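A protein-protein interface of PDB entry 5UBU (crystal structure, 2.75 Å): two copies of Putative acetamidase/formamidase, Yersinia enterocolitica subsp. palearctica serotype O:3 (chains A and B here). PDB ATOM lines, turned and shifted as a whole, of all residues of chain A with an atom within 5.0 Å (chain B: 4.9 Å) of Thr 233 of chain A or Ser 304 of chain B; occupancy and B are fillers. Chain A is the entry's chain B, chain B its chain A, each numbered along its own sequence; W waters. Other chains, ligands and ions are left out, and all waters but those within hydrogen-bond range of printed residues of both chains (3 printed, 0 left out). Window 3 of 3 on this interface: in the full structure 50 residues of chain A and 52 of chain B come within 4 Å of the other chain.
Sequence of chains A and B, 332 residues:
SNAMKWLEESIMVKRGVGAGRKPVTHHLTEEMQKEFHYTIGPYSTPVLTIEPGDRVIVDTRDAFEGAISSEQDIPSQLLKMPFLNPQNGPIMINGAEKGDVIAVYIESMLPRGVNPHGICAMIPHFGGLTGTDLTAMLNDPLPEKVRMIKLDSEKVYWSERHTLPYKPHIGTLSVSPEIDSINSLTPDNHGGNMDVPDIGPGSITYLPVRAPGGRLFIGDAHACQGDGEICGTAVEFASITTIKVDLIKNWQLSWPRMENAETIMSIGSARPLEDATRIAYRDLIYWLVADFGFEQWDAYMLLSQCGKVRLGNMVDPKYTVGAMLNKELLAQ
The backbone carbonyl oxygen (O) of Ile 230 of chain A is in hydrogen-bond range of the side-chain hydroxyl (OH) of Tyr 300 of chain B (3.3 Å).
The backbone carbonyl oxygen (O) of Ser 304 of chain B lies within hydrogen-bond range of the backbone NH (N) of Gly 226 of chain A, 2.8 Å away.
OG of Ser 304 of chain B sits at hydrogen-bond distance from N of Cys 231 of chain A (3.3 Å).
The side-chain hydroxyl (OG) of Ser 304 of chain B sits at hydrogen-bond distance from the backbone carbonyl oxygen (O) of Thr 233 of chain A (2.8 Å).
The side-chain amide nitrogen (NE2) of Gln 305 of chain B lies within hydrogen-bond range of the side-chain sulfur (SG) of Cys 120 of chain A (3.3 Å).
O of Gln 305 of chain B lies close to N of Gly 226 of chain A, 3.3 Å away.
The side-chain amide nitrogen (NE2) of Gln 305 of chain B is in hydrogen-bond range of the backbone carbonyl oxygen (O) of Thr 233 of chain A, 3.4 Å away.
The side-chain amide oxygen of Gln 305 of chain B is in hydrogen-bond range of the backbone NH of Val 235 of chain A, 3.1 Å away.
The backbone carbonyl oxygen of Gln 225 of chain A sits close to the backbone carbonyl oxygen of Gln 305 of chain B (3.4 Å).
Among the printed residues, merely in contact across the chains: Ala 234 of chain A with Gln 305 of chain B, Glu 229 of chain A with Ser 304 of chain B, Gly 226 of chain A with Gly 307 of chain B, Cys 231 of chain A with Tyr 300 of chain B, Ile 230 of chain A with Ser 304 of chain B, Ile 230 of chain A with Leu 303 of chain B, Gln 225 of chain A with Ser 304 of chain B, Met 122 of chain A with Met 301 of chain B, Gly 226 of chain A with Leu 303 of chain B, Gly 226 of chain A with Cys 306 of chain B and Met 122 of chain A with Tyr 300 of chain B.
Ala 121 of chain A touches none of the printed residues of chain B.
Printed residues of chain B within 4 Å of Gln 225 of chain A: Ser 304 (3.7 Å) and Gln 305 (3.2 Å).
Printed residues of chain B within 4 Å of Gly 226 of chain A: Leu 303 (3.8 Å), Ser 304 (2.8 Å), Gln 305 (3.3 Å), Cys 306 (3.9 Å) and Gly 307 (3.4 Å).
Gly 232 of chain A touches none of the printed residues of chain B.
Printed residues of chain B within 4 Å of Thr 233 of chain A: Ser 304 (2.8 Å) and Gln 305 (3.4 Å).
Of the printed residues of chain A, Tyr 300 of chain B touches Met 122 (3.9 Å), Ile 230 (3.3 Å) and Cys 231 (3.4 Å).
Printed residues of chain A within 4 Å of Met 301 of chain B: Met 122 (3.8 Å).
Of the printed residues of chain A, Ser 304 of chain B touches Gln 225 (3.7 Å), Gly 226 (2.8 Å), Glu 229 (3.3 Å), Ile 230 (3.6 Å), Cys 231 (3.3 Å) and Thr 233 (2.8 Å).
Printed residues of chain A within 4 Å of Cys 306 of chain B: Gly 226 (3.9 Å).
The nearest printed residue of chain A that does not touch Ser 304 of chain B is Gly 232 of chain A (4.3 Å).
The nearest printed residue of chain A that does not touch Leu 303 of chain B is Glu 229 of chain A (5.7 Å).
No position is printed for both chains.
Of the 20 pairs that touch across the chains among the printed residues, none has its exchanged pair printed and touching as well.
Water W3 bridges the side-chain hydroxyl (OH) of Tyr 300 of chain B and the backbone carbonyl oxygen (O) of Cys 231 of chain A.
Water W2 lies within hydrogen-bond range of N of Gln 225 of chain A (2.8 Å) and O of Gln 305 of chain B (3.4 Å).
Water W1 lies within hydrogen-bond range of N of Glu 229 of chain A (2.9 Å), O of Leu 303 of chain B (3.0 Å), N of Ile 230 of chain A (3.1 Å) and O of Gly 226 of chain A (3.4 Å).
The backbone carbonyl oxygen of Met 301 of chain B is in hydrogen-bond range of the side-chain amide nitrogen of Gln 305 of chain B (3.3 Å).
The side-chain sulfur of Cys 306 of chain B lies within hydrogen-bond range of the backbone carbonyl oxygen of Leu 302 of chain B.
The side-chain sulfur (SG) of Cys 120 of chain A is in hydrogen-bond range of the side-chain sulfur (SG) of Cys 231 of chain A (3.7 Å).
The side-chain sulfur (SG) of Cys 120 of chain A lies within hydrogen-bond range of the side-chain hydroxyl (OG1) of Thr 233 of chain A (3.4 Å).
The backbone carbonyl oxygen (O) of Thr 233 of chain A is in hydrogen-bond range of the side-chain sulfur (SG) of Cys 231 of chain A, 3.3 Å away.
The side-chain carboxylate of Glu 236 of chain A is in hydrogen-bond range of the backbone NH of Ala 234 of chain A (3.1 Å).
Of the 16 printed residues of chain A, 10 touch a printed residue of chain B.
Hydrophobic or aromatic side chains of chain A within 4 Å of the printed part of chain B: Met 122, Ile 230, Ala 234 and Val 235.
Hydrophobic or aromatic side chains of chain B within 4 Å of the printed part of chain A: Tyr 300, Met 301 and Leu 303.
Among the printed residues, 20 pairs touch across the chains.
Among the printed residues, no Asp or Glu carboxylate lies within 4 Å of a Lys or Arg side-chain nitrogen of the other chain.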
ATOM      1  N   PHE A  64       0.112  -1.796   5.795  1.00  0.00           N
ATOM      2  CA  PHE A  64      -0.928  -2.833   5.814  1.00  0.00           C
ATOM      3  C   PHE A  64      -1.968  -2.606   6.916  1.00  0.00           C
ATOM      4  O   PHE A  64      -2.871  -3.421   7.100  1.00  0.00           O
ATOM      5  CB  PHE A  64      -0.264  -4.210   5.998  1.00  0.00           C
ATOM      6  CG  PHE A  64       0.979  -4.393   5.163  1.00  0.00           C
ATOM      7  CD1 PHE A  64       0.885  -4.474   3.772  1.00  0.00           C
ATOM      8  CD2 PHE A  64       2.241  -4.465   5.757  1.00  0.00           C
ATOM      9  CE1 PHE A  64       2.026  -4.630   2.994  1.00  0.00           C
ATOM     10  CE2 PHE A  64       3.372  -4.619   4.978  1.00  0.00           C
ATOM     11  CZ  PHE A  64       3.270  -4.698   3.596  1.00  0.00           C
ATOM     12  N   ILE A 119       7.967  -4.682   8.366  1.00  0.00           N
ATOM     13  CA  ILE A 119       7.493  -5.765   7.501  1.00  0.00           C
ATOM     14  C   ILE A 119       7.803  -5.539   6.035  1.00  0.00           C
ATOM     15  O   ILE A 119       7.511  -4.481   5.499  1.00  0.00           O
ATOM     16  CB  ILE A 119       5.957  -5.900   7.591  1.00  0.00           C
ATOM     17  CG1 ILE A 119       5.532  -6.232   9.031  1.00  0.00           C
ATOM     18  CG2 ILE A 119       5.453  -7.025   6.689  1.00  0.00           C
ATOM     19  CD1 ILE A 119       4.029  -6.120   9.279  1.00  0.00           C
ATOM     20  N   CYS A 120       8.396  -6.535   5.393  1.00  0.00           N
ATOM     21  CA  CYS A 120       8.653  -6.489   3.962  1.00  0.00           C
ATOM     22  C   CYS A 120       7.827  -7.637   3.407  1.00  0.00           C
ATOM     23  O   CYS A 120       7.779  -8.717   4.004  1.00  0.00           O
ATOM     24  CB  CYS A 120      10.123  -6.679   3.609  1.00  0.00           C
ATOM     25  SG  CYS A 120      10.400  -6.639   1.808  1.00  0.00           S
ATOM     26  N   ALA A 121       7.172  -7.411   2.272  1.00  0.00           N
ATOM     27  CA  ALA A 121       6.325  -8.438   1.683  1.00  0.00           C
ATOM     28  C   ALA A 121       6.337  -8.446   0.173  1.00  0.00           C
ATOM     29  O   ALA A 121       6.535  -7.412  -0.468  1.00  0.00           O
ATOM     30  CB  ALA A 121       4.891  -8.256   2.176  1.00  0.00           C
ATOM     31  N   MET A 122       6.124  -9.641  -0.372  1.00  0.00           N
ATOM     32  CA  MET A 122       6.048  -9.862  -1.802  1.00  0.00           C
ATOM     33  C   MET A 122       4.601 -10.156  -2.027  1.00  0.00           C
ATOM     34  O   MET A 122       4.127 -11.254  -1.764  1.00  0.00           O
ATOM     35  CB  MET A 122       6.923 -11.016  -2.245  1.00  0.00           C
ATOM     36  CG  MET A 122       8.338 -10.549  -2.550  1.00  0.00           C
ATOM     37  SD  MET A 122       9.486 -12.158  -2.761  1.00  0.00           S
ATOM     38  CE  MET A 122       8.840 -12.773  -4.499  1.00  0.00           C
ATOM     39  N   ILE A 123       3.881  -9.140  -2.477  1.00  0.00           N
ATOM     40  CA  ILE A 123       2.456  -9.231  -2.738  1.00  0.00           C
ATOM     41  C   ILE A 123       2.233  -9.743  -4.161  1.00  0.00           C
ATOM     42  O   ILE A 123       2.849  -9.229  -5.099  1.00  0.00           O
ATOM     43  CB  ILE A 123       1.805  -7.851  -2.559  1.00  0.00           C
ATOM     44  CG1 ILE A 123       2.109  -7.327  -1.141  1.00  0.00           C
ATOM     45  CG2 ILE A 123       0.306  -7.930  -2.838  1.00  0.00           C
ATOM     46  CD1 ILE A 123       1.631  -5.922  -0.855  1.00  0.00           C
ATOM     47  N   GLN A 225      14.923   1.786   2.538  1.00  0.00           N
ATOM     48  CA  GLN A 225      14.400   1.504   1.192  1.00  0.00           C
ATOM     49  C   GLN A 225      15.461   1.635   0.117  1.00  0.00           C
ATOM     50  O   GLN A 225      16.260   2.575   0.129  1.00  0.00           O
ATOM     51  CB  GLN A 225      13.236   2.432   0.814  1.00  0.00           C
ATOM     52  CG  GLN A 225      12.636   2.162  -0.570  1.00  0.00           C
ATOM     53  CD  GLN A 225      11.669   3.223  -1.019  1.00  0.00           C
ATOM     54  OE1 GLN A 225      10.738   3.580  -0.304  1.00  0.00           O
ATOM     55  NE2 GLN A 225      11.873   3.714  -2.225  1.00  0.00           N
ATOM     56  N   GLY A 226      15.421   0.706  -0.839  1.00  0.00           N
ATOM     57  CA  GLY A 226      16.335   0.730  -1.962  1.00  0.00           C
ATOM     58  C   GLY A 226      15.771   1.604  -3.080  1.00  0.00           C
ATOM     59  O   GLY A 226      14.575   1.939  -3.093  1.00  0.00           O
ATOM     60  N   GLU A 229      12.470   0.479  -4.869  1.00  0.00           N
ATOM     61  CA  GLU A 229      11.623  -0.330  -3.965  1.00  0.00           C
ATOM     62  C   GLU A 229      11.180  -1.551  -4.781  1.00  0.00           C
ATOM     63  O   GLU A 229      10.010  -1.967  -4.732  1.00  0.00           O
ATOM     64  CB  GLU A 229      10.434   0.522  -3.517  1.00  0.00           C
ATOM     65  CG  GLU A 229       9.615  -0.009  -2.350  1.00  0.00           C
ATOM     66  CD  GLU A 229       8.393   0.853  -2.067  1.00  0.00           C
ATOM     67  OE1 GLU A 229       7.858   1.443  -3.025  1.00  0.00           O
ATOM     68  OE2 GLU A 229       7.942   0.921  -0.895  1.00  0.00           O
ATOM     69  N   ILE A 230      12.140  -2.124  -5.509  1.00  0.00           N
ATOM     70  CA  ILE A 230      11.841  -3.197  -6.458  1.00  0.00           C
ATOM     71  C   ILE A 230      10.926  -4.362  -6.132  1.00  0.00           C
ATOM     72  O   ILE A 230      10.209  -4.772  -7.047  1.00  0.00           O
ATOM     73  CB  ILE A 230      13.053  -3.804  -7.166  1.00  0.00           C
ATOM     74  CG1 ILE A 230      14.130  -4.086  -6.153  1.00  0.00           C
ATOM     75  CG2 ILE A 230      13.457  -2.930  -8.313  1.00  0.00           C
ATOM     76  CD1 ILE A 230      15.211  -4.972  -6.707  1.00  0.00           C
ATOM     77  N   CYS A 231      10.880  -4.892  -4.901  1.00  0.00           N
ATOM     78  CA  CYS A 231       9.965  -6.032  -4.644  1.00  0.00           C
ATOM     79  C   CYS A 231       8.518  -5.604  -4.402  1.00  0.00           C
ATOM     80  O   CYS A 231       7.633  -6.460  -4.297  1.00  0.00           O
ATOM     81  CB  CYS A 231      10.441  -6.908  -3.492  1.00  0.00           C
ATOM     82  SG  CYS A 231      10.101  -6.272  -1.845  1.00  0.00           S
ATOM     83  N   GLY A 232       8.284  -4.287  -4.309  1.00  0.00           N
ATOM     84  CA  GLY A 232       6.948  -3.737  -4.082  1.00  0.00           C
ATOM     85  C   GLY A 232       6.833  -3.040  -2.745  1.00  0.00           C
ATOM     86  O   GLY A 232       6.061  -2.081  -2.606  1.00  0.00           O
ATOM     87  N   THR A 233       7.594  -3.521  -1.756  1.00  0.00           N
ATOM     88  CA  THR A 233       7.574  -2.937  -0.413  1.00  0.00           C
ATOM     89  C   THR A 233       8.969  -2.755   0.168  1.00  0.00           C
ATOM     90  O   THR A 233       9.907  -3.465  -0.177  1.00  0.00           O
ATOM     91  CB  THR A 233       6.791  -3.828   0.596  1.00  0.00           C
ATOM     92  OG1 THR A 233       7.519  -5.030   0.871  1.00  0.00           O
ATOM     93  CG2 THR A 233       5.408  -4.184   0.075  1.00  0.00           C
ATOM     94  N   ALA A 234       9.074  -1.795   1.073  1.00  0.00           N
ATOM     95  CA  ALA A 234      10.303  -1.511   1.785  1.00  0.00           C
ATOM     96  C   ALA A 234      10.097  -2.199   3.132  1.00  0.00           C
ATOM     97  O   ALA A 234       9.373  -3.193   3.200  1.00  0.00           O
ATOM     98  CB  ALA A 234      10.460  -0.013   1.955  1.00  0.00           C
ATOM     99  N   VAL A 235      10.761  -1.721   4.184  1.00  0.00           N
ATOM    100  CA  VAL A 235      10.538  -2.271   5.521  1.00  0.00           C
ATOM    101  C   VAL A 235       9.468  -1.345   6.100  1.00  0.00           C
ATOM    102  O   VAL A 235       9.771  -0.284   6.625  1.00  0.00           O
ATOM    103  CB  VAL A 235      11.817  -2.333   6.388  1.00  0.00           C
ATOM    104  CG1 VAL A 235      11.478  -2.710   7.826  1.00  0.00           C
ATOM    105  CG2 VAL A 235      12.808  -3.330   5.790  1.00  0.00           C
ATOM    106  N   GLU A 236       8.214  -1.767   5.958  1.00  0.00           N
ATOM    107  CA  GLU A 236       7.053  -1.006   6.409  1.00  0.00           C
ATOM    108  C   GLU A 236       6.901  -1.074   7.927  1.00  0.00           C
ATOM    109  O   GLU A 236       6.940  -2.174   8.504  1.00  0.00           O
ATOM    110  CB  GLU A 236       5.788  -1.610   5.794  1.00  0.00           C
ATOM    111  CG  GLU A 236       5.826  -1.859   4.290  1.00  0.00           C
ATOM    112  CD  GLU A 236       5.981  -0.604   3.465  1.00  0.00           C
ATOM    113  OE1 GLU A 236       6.387  -0.735   2.284  1.00  0.00           O
ATOM    114  OE2 GLU A 236       5.699   0.502   3.977  1.00  0.00           O
ATOM    115  N   TYR B 300      16.137 -10.376  -3.775  1.00  0.00           N
ATOM    116  CA  TYR B 300      15.123  -9.488  -4.351  1.00  0.00           C
ATOM    117  C   TYR B 300      14.554  -8.537  -3.291  1.00  0.00           C
ATOM    118  O   TYR B 300      14.514  -7.320  -3.493  1.00  0.00           O
ATOM    119  CB  TYR B 300      14.037 -10.357  -4.991  1.00  0.00           C
ATOM    120  CG  TYR B 300      12.844  -9.664  -5.625  1.00  0.00           C
ATOM    121  CD1 TYR B 300      12.995  -8.648  -6.554  1.00  0.00           C
ATOM    122  CD2 TYR B 300      11.566 -10.145  -5.400  1.00  0.00           C
ATOM    123  CE1 TYR B 300      11.893  -8.057  -7.157  1.00  0.00           C
ATOM    124  CE2 TYR B 300      10.460  -9.581  -6.004  1.00  0.00           C
ATOM    125  CZ  TYR B 300      10.622  -8.545  -6.886  1.00  0.00           C
ATOM    126  OH  TYR B 300       9.499  -8.000  -7.468  1.00  0.00           O
ATOM    127  N   MET B 301      14.162  -9.092  -2.154  1.00  0.00           N
ATOM    128  CA  MET B 301      13.601  -8.298  -1.066  1.00  0.00           C
ATOM    129  C   MET B 301      14.655  -7.466  -0.391  1.00  0.00           C
ATOM    130  O   MET B 301      14.357  -6.385   0.093  1.00  0.00           O
ATOM    131  CB  MET B 301      12.903  -9.200  -0.058  1.00  0.00           C
ATOM    132  CG  MET B 301      11.687  -9.868  -0.692  1.00  0.00           C
ATOM    133  SD  MET B 301      10.746 -10.944   0.658  1.00  0.00           S
ATOM    134  CE  MET B 301      11.967 -12.470   0.969  1.00  0.00           C
ATOM    135  N   LEU B 302      15.895  -7.947  -0.352  1.00  0.00           N
ATOM    136  CA  LEU B 302      16.986  -7.184   0.272  1.00  0.00           C
ATOM    137  C   LEU B 302      17.331  -5.960  -0.574  1.00  0.00           C
ATOM    138  O   LEU B 302      17.566  -4.878  -0.028  1.00  0.00           O
ATOM    139  CB  LEU B 302      18.252  -8.036   0.475  1.00  0.00           C
ATOM    140  CG  LEU B 302      19.411  -7.310   1.184  1.00  0.00           C
ATOM    141  CD1 LEU B 302      19.031  -6.922   2.610  1.00  0.00           C
ATOM    142  CD2 LEU B 302      20.669  -8.157   1.199  1.00  0.00           C
ATOM    143  N   LEU B 303      17.375  -6.135  -1.899  1.00  0.00           N
ATOM    144  CA  LEU B 303      17.671  -5.024  -2.815  1.00  0.00           C
ATOM    145  C   LEU B 303      16.577  -3.977  -2.792  1.00  0.00           C
ATOM    146  O   LEU B 303      16.793  -2.848  -3.210  1.00  0.00           O
ATOM    147  CB  LEU B 303      17.889  -5.509  -4.246  1.00  0.00           C
ATOM    148  CG  LEU B 303      19.202  -6.235  -4.485  1.00  0.00           C
ATOM    149  CD1 LEU B 303      19.244  -6.790  -5.899  1.00  0.00           C
ATOM    150  CD2 LEU B 303      20.382  -5.306  -4.223  1.00  0.00           C
ATOM    151  N   SER B 304      15.400  -4.366  -2.312  1.00  0.00           N
ATOM    152  CA  SER B 304      14.290  -3.444  -2.183  1.00  0.00           C
ATOM    153  C   SER B 304      14.561  -2.521  -0.981  1.00  0.00           C
ATOM    154  O   SER B 304      13.817  -1.567  -0.746  1.00  0.00           O
ATOM    155  CB  SER B 304      12.985  -4.220  -1.998  1.00  0.00           C
ATOM    156  OG  SER B 304      11.863  -3.367  -2.108  1.00  0.00           O
ATOM    157  N   GLN B 305      15.639  -2.805  -0.240  1.00  0.00           N
ATOM    158  CA  GLN B 305      16.039  -2.022   0.929  1.00  0.00           C
ATOM    159  C   GLN B 305      17.430  -1.368   0.762  1.00  0.00           C
ATOM    160  O   GLN B 305      17.681  -0.313   1.346  1.00  0.00           O
ATOM    161  CB  GLN B 305      16.103  -2.921   2.181  1.00  0.00           C
ATOM    162  CG  GLN B 305      14.986  -3.940   2.341  1.00  0.00           C
ATOM    163  CD  GLN B 305      13.596  -3.343   2.269  1.00  0.00           C
ATOM    164  OE1 GLN B 305      13.374  -2.185   2.646  1.00  0.00           O
ATOM    165  NE2 GLN B 305      12.637  -4.146   1.804  1.00  0.00           N
ATOM    166  N   CYS B 306      18.310  -1.992  -0.031  1.00  0.00           N
ATOM    167  CA  CYS B 306      19.706  -1.531  -0.201  1.00  0.00           C
ATOM    168  C   CYS B 306      20.182  -1.238  -1.604  1.00  0.00           C
ATOM    169  O   CYS B 306      21.277  -0.693  -1.773  1.00  0.00           O
ATOM    170  CB  CYS B 306      20.631  -2.622   0.309  1.00  0.00           C
ATOM    171  SG  CYS B 306      20.216  -3.107   1.970  1.00  0.00           S
ATOM    172  N   GLY B 307      19.411  -1.638  -2.604  1.00  0.00           N
ATOM    173  CA  GLY B 307      19.814  -1.404  -3.972  1.00  0.00           C
ATOM    174  C   GLY B 307      19.951   0.073  -4.290  1.00  0.00           C
ATOM    175  O   GLY B 307      19.180   0.890  -3.799  1.00  0.00           O
HETATM  176  O   HOH W   1      14.892  -1.091  -4.634  1.00  0.00           O
HETATM  177  O   HOH W   2      17.519   2.613   3.001  1.00  0.00           O
HETATM  178  O   HOH W   3       7.265  -8.658  -6.046  1.00  0.00           O
